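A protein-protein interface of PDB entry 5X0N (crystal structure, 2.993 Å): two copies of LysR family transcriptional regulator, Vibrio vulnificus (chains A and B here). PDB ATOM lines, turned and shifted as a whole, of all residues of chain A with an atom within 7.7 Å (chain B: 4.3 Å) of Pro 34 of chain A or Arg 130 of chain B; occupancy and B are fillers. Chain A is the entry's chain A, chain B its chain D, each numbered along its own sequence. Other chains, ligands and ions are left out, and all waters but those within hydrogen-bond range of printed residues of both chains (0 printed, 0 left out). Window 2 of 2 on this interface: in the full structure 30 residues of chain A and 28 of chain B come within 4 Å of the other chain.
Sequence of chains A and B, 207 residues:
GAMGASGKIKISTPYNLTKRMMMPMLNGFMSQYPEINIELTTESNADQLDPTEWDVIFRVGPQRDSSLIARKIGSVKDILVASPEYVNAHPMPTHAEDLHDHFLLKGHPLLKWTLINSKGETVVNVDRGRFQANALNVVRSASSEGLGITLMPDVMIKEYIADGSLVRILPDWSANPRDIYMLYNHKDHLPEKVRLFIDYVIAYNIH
The backbone NH (N) of Ile 38 of chain A lies within hydrogen-bond range of the backbone carbonyl oxygen (O) of Arg 130 of chain B.
The backbone carbonyl oxygen (O) of Met 30 of chain A sits at hydrogen-bond distance from the guanidinium group (NH2) of Arg 130 of chain B (2.8 Å).
Of the 7 printed residues of chain B, 5 touch a printed residue of chain A.
Hydrophobic or aromatic side chains of chain B that line the printed part of chain A: Phe 131 and Leu 147.
Printed residues of chain A that touch a printed residue of chain B: Lys 8, Asn 27, Met 30, Pro 34, Ile 36, Asn 37 and Ile 38.
Among the printed residues, 11 pairs touch across the chains.
Among the printed residues, no Asp or Glu carboxylate lies within 4 Å of a Lys or Arg side-chain nitrogen of the other chain.
Of the printed residues of chain B, Lys 8 of chain A touches Arg 128.
Of the printed residues of chain B, Asn 27 of chain A touches Leu 147 (3.6 Å).
Glu 35 of chain A touches none of the printed residues of chain B.
Printed residues of chain B within 4 Å of Asn 37 of chain A: Gly 129 and Arg 130.
Of chain A, only Asn 37 comes within 4 Å of Gly 129 of chain B.
Arg 130 of chain B touches just these residues of chain A: Met 30 (2.8 Å), Pro 34 (3.8 Å), Ile 36 (3.95 Å), Asn 37 (3.5 Å) and Ile 38 (3.3 Å).
The nearest residue of chain B that does not touch Pro 34 of chain A is Phe 103 of chain B (4.1 Å).
No position is printed for both chains.
Of the 11 pairs that touch across the chains among the printed residues, none has its exchanged pair printed and touching as well.
Among the printed residues, merely in contact across the chains: Lys 8 of chain A with Arg 128 of chain B, Ile 38 of chain A with Phe 131 of chain B, Met 30 of chain A with Phe 131 of chain B, Asn 37 of chain A with Arg 130 of chain B, Asn 27 of chain A with Leu 147 of chain B, Pro 34 of chain A with Arg 130 of chain B, Asn 37 of chain A with Gly 129 of chain B, Met 30 of chain A with Leu 147 of chain B and Ile 36 of chain A with Arg 130 of chain B.
O of Asn 27 of chain A lies close to OG of Ser 31 of chain A (3.5 Å).
NH1 of Arg 130 of chain B sits at hydrogen-bond distance from O of Leu 147 of chain B (2.9 Å).
The backbone carbonyl oxygen (O) of Leu 104 of chain B lies within hydrogen-bond range of the backbone NH (N) of Arg 130 of chain B (2.9 Å).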
ATOM      1  N   LYS A   8      16.971   8.593  23.240  1.00  0.00           N
ATOM      2  CA  LYS A   8      18.326   8.640  23.776  1.00  0.00           C
ATOM      3  C   LYS A   8      19.250   7.707  23.003  1.00  0.00           C
ATOM      4  O   LYS A   8      18.888   6.568  22.708  1.00  0.00           O
ATOM      5  CB  LYS A   8      18.329   8.272  25.263  1.00  0.00           C
ATOM      6  CG  LYS A   8      19.714   8.241  25.895  1.00  0.00           C
ATOM      7  CD  LYS A   8      19.635   8.061  27.403  1.00  0.00           C
ATOM      8  CE  LYS A   8      19.511   9.398  28.117  1.00  0.00           C
ATOM      9  NZ  LYS A   8      19.747   9.267  29.581  1.00  0.00           N
ATOM     10  N   ASN A  27      30.584  16.879  22.945  1.00  0.00           N
ATOM     11  CA  ASN A  27      30.068  18.152  23.442  1.00  0.00           C
ATOM     12  C   ASN A  27      29.590  19.041  22.302  1.00  0.00           C
ATOM     13  O   ASN A  27      28.613  19.785  22.452  1.00  0.00           O
ATOM     14  CB  ASN A  27      31.139  18.871  24.262  1.00  0.00           C
ATOM     15  CG  ASN A  27      31.437  18.173  25.572  1.00  0.00           C
ATOM     16  OD1 ASN A  27      32.407  17.429  25.684  1.00  0.00           O
ATOM     17  ND2 ASN A  27      30.597  18.410  26.571  1.00  0.00           N
ATOM     18  N   PHE A  29      28.255  17.948  19.542  1.00  0.00           N
ATOM     19  CA  PHE A  29      27.044  17.380  18.958  1.00  0.00           C
ATOM     20  C   PHE A  29      25.806  17.798  19.743  1.00  0.00           C
ATOM     21  O   PHE A  29      24.799  18.214  19.157  1.00  0.00           O
ATOM     22  CB  PHE A  29      27.159  15.856  18.896  1.00  0.00           C
ATOM     23  CG  PHE A  29      25.874  15.165  18.542  1.00  0.00           C
ATOM     24  CD1 PHE A  29      25.420  15.143  17.232  1.00  0.00           C
ATOM     25  CD2 PHE A  29      25.123  14.532  19.517  1.00  0.00           C
ATOM     26  CE1 PHE A  29      24.238  14.506  16.905  1.00  0.00           C
ATOM     27  CE2 PHE A  29      23.941  13.893  19.197  1.00  0.00           C
ATOM     28  CZ  PHE A  29      23.498  13.880  17.889  1.00  0.00           C
ATOM     29  N   MET A  30      25.858  17.691  21.075  1.00  0.00           N
ATOM     30  CA  MET A  30      24.739  18.154  21.890  1.00  0.00           C
ATOM     31  C   MET A  30      24.580  19.665  21.815  1.00  0.00           C
ATOM     32  O   MET A  30      23.471  20.180  21.987  1.00  0.00           O
ATOM     33  CB  MET A  30      24.922  17.708  23.342  1.00  0.00           C
ATOM     34  CG  MET A  30      25.861  16.535  23.503  1.00  0.00           C
ATOM     35  SD  MET A  30      25.511  15.602  24.999  1.00  0.00           S
ATOM     36  CE  MET A  30      26.084  16.760  26.232  1.00  0.00           C
ATOM     37  N   SER A  31      25.672  20.387  21.561  1.00  0.00           N
ATOM     38  CA  SER A  31      25.572  21.822  21.339  1.00  0.00           C
ATOM     39  C   SER A  31      24.852  22.149  20.037  1.00  0.00           C
ATOM     40  O   SER A  31      24.350  23.268  19.883  1.00  0.00           O
ATOM     41  CB  SER A  31      26.967  22.456  21.341  1.00  0.00           C
ATOM     42  OG  SER A  31      27.653  22.186  20.131  1.00  0.00           O
ATOM     43  N   GLN A  32      24.788  21.201  19.103  1.00  0.00           N
ATOM     44  CA  GLN A  32      24.058  21.375  17.855  1.00  0.00           C
ATOM     45  C   GLN A  32      22.719  20.654  17.840  1.00  0.00           C
ATOM     46  O   GLN A  32      21.944  20.844  16.897  1.00  0.00           O
ATOM     47  CB  GLN A  32      24.898  20.883  16.672  1.00  0.00           C
ATOM     48  CG  GLN A  32      26.110  21.734  16.384  1.00  0.00           C
ATOM     49  CD  GLN A  32      25.826  22.845  15.396  1.00  0.00           C
ATOM     50  OE1 GLN A  32      24.957  22.719  14.535  1.00  0.00           O
ATOM     51  NE2 GLN A  32      26.564  23.944  15.513  1.00  0.00           N
ATOM     52  N   TYR A  33      22.435  19.828  18.843  1.00  0.00           N
ATOM     53  CA  TYR A  33      21.196  19.051  18.902  1.00  0.00           C
ATOM     54  C   TYR A  33      20.736  18.979  20.350  1.00  0.00           C
ATOM     55  O   TYR A  33      21.023  18.013  21.067  1.00  0.00           O
ATOM     56  CB  TYR A  33      21.396  17.650  18.316  1.00  0.00           C
ATOM     57  CG  TYR A  33      21.791  17.631  16.855  1.00  0.00           C
ATOM     58  CD1 TYR A  33      20.832  17.516  15.857  1.00  0.00           C
ATOM     59  CD2 TYR A  33      23.124  17.717  16.474  1.00  0.00           C
ATOM     60  CE1 TYR A  33      21.188  17.494  14.520  1.00  0.00           C
ATOM     61  CE2 TYR A  33      23.489  17.697  15.140  1.00  0.00           C
ATOM     62  CZ  TYR A  33      22.519  17.586  14.168  1.00  0.00           C
ATOM     63  OH  TYR A  33      22.882  17.565  12.841  1.00  0.00           O
ATOM     64  N   PRO A  34      20.017  20.003  20.823  1.00  0.00           N
ATOM     65  CA  PRO A  34      19.537  19.977  22.215  1.00  0.00           C
ATOM     66  C   PRO A  34      18.458  18.938  22.471  1.00  0.00           C
ATOM     67  O   PRO A  34      18.276  18.537  23.628  1.00  0.00           O
ATOM     68  CB  PRO A  34      19.004  21.400  22.431  1.00  0.00           C
ATOM     69  CG  PRO A  34      18.686  21.900  21.058  1.00  0.00           C
ATOM     70  CD  PRO A  34      19.696  21.270  20.144  1.00  0.00           C
ATOM     71  N   GLU A  35      17.742  18.490  21.442  1.00  0.00           N
ATOM     72  CA  GLU A  35      16.702  17.484  21.615  1.00  0.00           C
ATOM     73  C   GLU A  35      17.259  16.078  21.800  1.00  0.00           C
ATOM     74  O   GLU A  35      16.478  15.145  22.020  1.00  0.00           O
ATOM     75  CB  GLU A  35      15.749  17.500  20.416  1.00  0.00           C
ATOM     76  CG  GLU A  35      15.020  18.819  20.218  1.00  0.00           C
ATOM     77  CD  GLU A  35      13.533  18.634  19.976  1.00  0.00           C
ATOM     78  OE1 GLU A  35      13.148  18.312  18.832  1.00  0.00           O
ATOM     79  OE2 GLU A  35      12.748  18.812  20.932  1.00  0.00           O
ATOM     80  N   ILE A  36      18.574  15.902  21.724  1.00  0.00           N
ATOM     81  CA  ILE A  36      19.201  14.590  21.819  1.00  0.00           C
ATOM     82  C   ILE A  36      19.725  14.399  23.235  1.00  0.00           C
ATOM     83  O   ILE A  36      20.540  15.196  23.718  1.00  0.00           O
ATOM     84  CB  ILE A  36      20.331  14.429  20.792  1.00  0.00           C
ATOM     85  CG1 ILE A  36      19.789  14.584  19.370  1.00  0.00           C
ATOM     86  CG2 ILE A  36      21.015  13.080  20.961  1.00  0.00           C
ATOM     87  CD1 ILE A  36      18.637  13.664  19.056  1.00  0.00           C
ATOM     88  N   ASN A  37      19.256  13.348  23.898  1.00  0.00           N
ATOM     89  CA  ASN A  37      19.814  12.906  25.166  1.00  0.00           C
ATOM     90  C   ASN A  37      20.798  11.774  24.901  1.00  0.00           C
ATOM     91  O   ASN A  37      20.519  10.868  24.111  1.00  0.00           O
ATOM     92  CB  ASN A  37      18.714  12.443  26.122  1.00  0.00           C
ATOM     93  CG  ASN A  37      17.675  13.519  26.375  1.00  0.00           C
ATOM     94  OD1 ASN A  37      18.006  14.644  26.756  1.00  0.00           O
ATOM     95  ND2 ASN A  37      16.409  13.181  26.162  1.00  0.00           N
ATOM     96  N   ILE A  38      21.957  11.841  25.552  1.00  0.00           N
ATOM     97  CA  ILE A  38      23.046  10.899  25.327  1.00  0.00           C
ATOM     98  C   ILE A  38      23.402  10.235  26.646  1.00  0.00           C
ATOM     99  O   ILE A  38      23.573  10.916  27.665  1.00  0.00           O
ATOM    100  CB  ILE A  38      24.282  11.588  24.721  1.00  0.00           C
ATOM    101  CG1 ILE A  38      23.911  12.342  23.442  1.00  0.00           C
ATOM    102  CG2 ILE A  38      25.382  10.566  24.443  1.00  0.00           C
ATOM    103  CD1 ILE A  38      25.110  12.823  22.653  1.00  0.00           C
ATOM    104  N   GLU A  39      23.518   8.913  26.628  1.00  0.00           N
ATOM    105  CA  GLU A  39      24.053   8.165  27.753  1.00  0.00           C
ATOM    106  C   GLU A  39      25.369   7.537  27.321  1.00  0.00           C
ATOM    107  O   GLU A  39      25.440   6.902  26.262  1.00  0.00           O
ATOM    108  CB  GLU A  39      23.077   7.079  28.220  1.00  0.00           C
ATOM    109  CG  GLU A  39      23.695   6.147  29.245  1.00  0.00           C
ATOM    110  CD  GLU A  39      23.226   4.723  29.106  1.00  0.00           C
ATOM    111  OE1 GLU A  39      23.954   3.913  28.503  1.00  0.00           O
ATOM    112  OE2 GLU A  39      22.133   4.418  29.617  1.00  0.00           O
ATOM    113  N   PHE B 103      18.379  22.072  31.646  1.00  0.00           N
ATOM    114  CA  PHE B 103      19.202  20.931  31.276  1.00  0.00           C
ATOM    115  C   PHE B 103      20.020  20.495  32.484  1.00  0.00           C
ATOM    116  O   PHE B 103      20.673  21.319  33.132  1.00  0.00           O
ATOM    117  CB  PHE B 103      20.128  21.285  30.111  1.00  0.00           C
ATOM    118  CG  PHE B 103      19.407  21.671  28.852  1.00  0.00           C
ATOM    119  CD1 PHE B 103      18.777  20.713  28.074  1.00  0.00           C
ATOM    120  CD2 PHE B 103      19.366  22.994  28.442  1.00  0.00           C
ATOM    121  CE1 PHE B 103      18.118  21.069  26.912  1.00  0.00           C
ATOM    122  CE2 PHE B 103      18.709  23.357  27.281  1.00  0.00           C
ATOM    123  CZ  PHE B 103      18.083  22.392  26.516  1.00  0.00           C
ATOM    124  N   LEU B 104      19.981  19.203  32.791  1.00  0.00           N
ATOM    125  CA  LEU B 104      20.730  18.643  33.905  1.00  0.00           C
ATOM    126  C   LEU B 104      21.748  17.641  33.379  1.00  0.00           C
ATOM    127  O   LEU B 104      21.448  16.853  32.477  1.00  0.00           O
ATOM    128  CB  LEU B 104      19.802  17.969  34.920  1.00  0.00           C
ATOM    129  CG  LEU B 104      18.706  18.853  35.523  1.00  0.00           C
ATOM    130  CD1 LEU B 104      17.798  18.047  36.439  1.00  0.00           C
ATOM    131  CD2 LEU B 104      19.300  20.050  36.253  1.00  0.00           C
ATOM    132  N   ARG B 128      15.925  12.370  33.644  1.00  0.00           N
ATOM    133  CA  ARG B 128      16.748  11.914  32.530  1.00  0.00           C
ATOM    134  C   ARG B 128      17.495  13.138  32.012  1.00  0.00           C
ATOM    135  O   ARG B 128      16.950  13.928  31.235  1.00  0.00           O
ATOM    136  CB  ARG B 128      15.899  11.267  31.437  1.00  0.00           C
ATOM    137  CG  ARG B 128      16.702  10.460  30.429  1.00  0.00           C
ATOM    138  CD  ARG B 128      15.882  10.130  29.190  1.00  0.00           C
ATOM    139  NE  ARG B 128      14.603   9.509  29.522  1.00  0.00           N
ATOM    140  CZ  ARG B 128      14.428   8.204  29.699  1.00  0.00           C
ATOM    141  NH1 ARG B 128      15.454   7.371  29.576  1.00  0.00           N
ATOM    142  NH2 ARG B 128      13.227   7.727  29.999  1.00  0.00           N
ATOM    143  N   GLY B 129      18.738  13.298  32.457  1.00  0.00           N
ATOM    144  CA  GLY B 129      19.500  14.474  32.097  1.00  0.00           C
ATOM    145  C   GLY B 129      19.849  14.519  30.623  1.00  0.00           C
ATOM    146  O   GLY B 129      19.845  13.511  29.915  1.00  0.00           O
ATOM    147  N   ARG B 130      20.152  15.734  30.155  1.00  0.00           N
ATOM    148  CA  ARG B 130      20.603  15.911  28.779  1.00  0.00           C
ATOM    149  C   ARG B 130      21.826  15.055  28.481  1.00  0.00           C
ATOM    150  O   ARG B 130      22.026  14.632  27.336  1.00  0.00           O
ATOM    151  CB  ARG B 130      20.907  17.389  28.516  1.00  0.00           C
ATOM    152  CG  ARG B 130      21.294  17.714  27.080  1.00  0.00           C
ATOM    153  CD  ARG B 130      22.444  18.710  27.030  1.00  0.00           C
ATOM    154  NE  ARG B 130      22.523  19.398  25.743  1.00  0.00           N
ATOM    155  CZ  ARG B 130      22.261  20.690  25.568  1.00  0.00           C
ATOM    156  NH1 ARG B 130      21.901  21.442  26.599  1.00  0.00           N
ATOM    157  NH2 ARG B 130      22.360  21.231  24.362  1.00  0.00           N
ATOM    158  N   PHE B 131      22.639  14.774  29.498  1.00  0.00           N
ATOM    159  CA  PHE B 131      23.836  13.956  29.331  1.00  0.00           C
ATOM    160  C   PHE B 131      24.091  13.221  30.638  1.00  0.00           C
ATOM    161  O   PHE B 131      24.424  13.848  31.649  1.00  0.00           O
ATOM    162  CB  PHE B 131      25.033  14.818  28.940  1.00  0.00           C
ATOM    163  CG  PHE B 131      26.305  14.045  28.752  1.00  0.00           C
ATOM    164  CD1 PHE B 131      26.444  13.159  27.697  1.00  0.00           C
ATOM    165  CD2 PHE B 131      27.366  14.216  29.623  1.00  0.00           C
ATOM    166  CE1 PHE B 131      27.615  12.449  27.520  1.00  0.00           C
ATOM    167  CE2 PHE B 131      28.541  13.510  29.452  1.00  0.00           C
ATOM    168  CZ  PHE B 131      28.665  12.625  28.399  1.00  0.00           C
ATOM    169  N   LEU B 147      26.274  23.210  28.795  1.00  0.00           N
ATOM    170  CA  LEU B 147      25.162  22.434  28.263  1.00  0.00           C
ATOM    171  C   LEU B 147      24.216  21.947  29.350  1.00  0.00           C
ATOM    172  O   LEU B 147      23.386  21.071  29.088  1.00  0.00           O
ATOM    173  CB  LEU B 147      25.692  21.246  27.451  1.00  0.00           C
ATOM    174  CG  LEU B 147      26.895  21.603  26.582  1.00  0.00           C
ATOM    175  CD1 LEU B 147      27.601  20.353  26.079  1.00  0.00           C
ATOM    176  CD2 LEU B 147      26.456  22.492  25.430  1.00  0.00           C
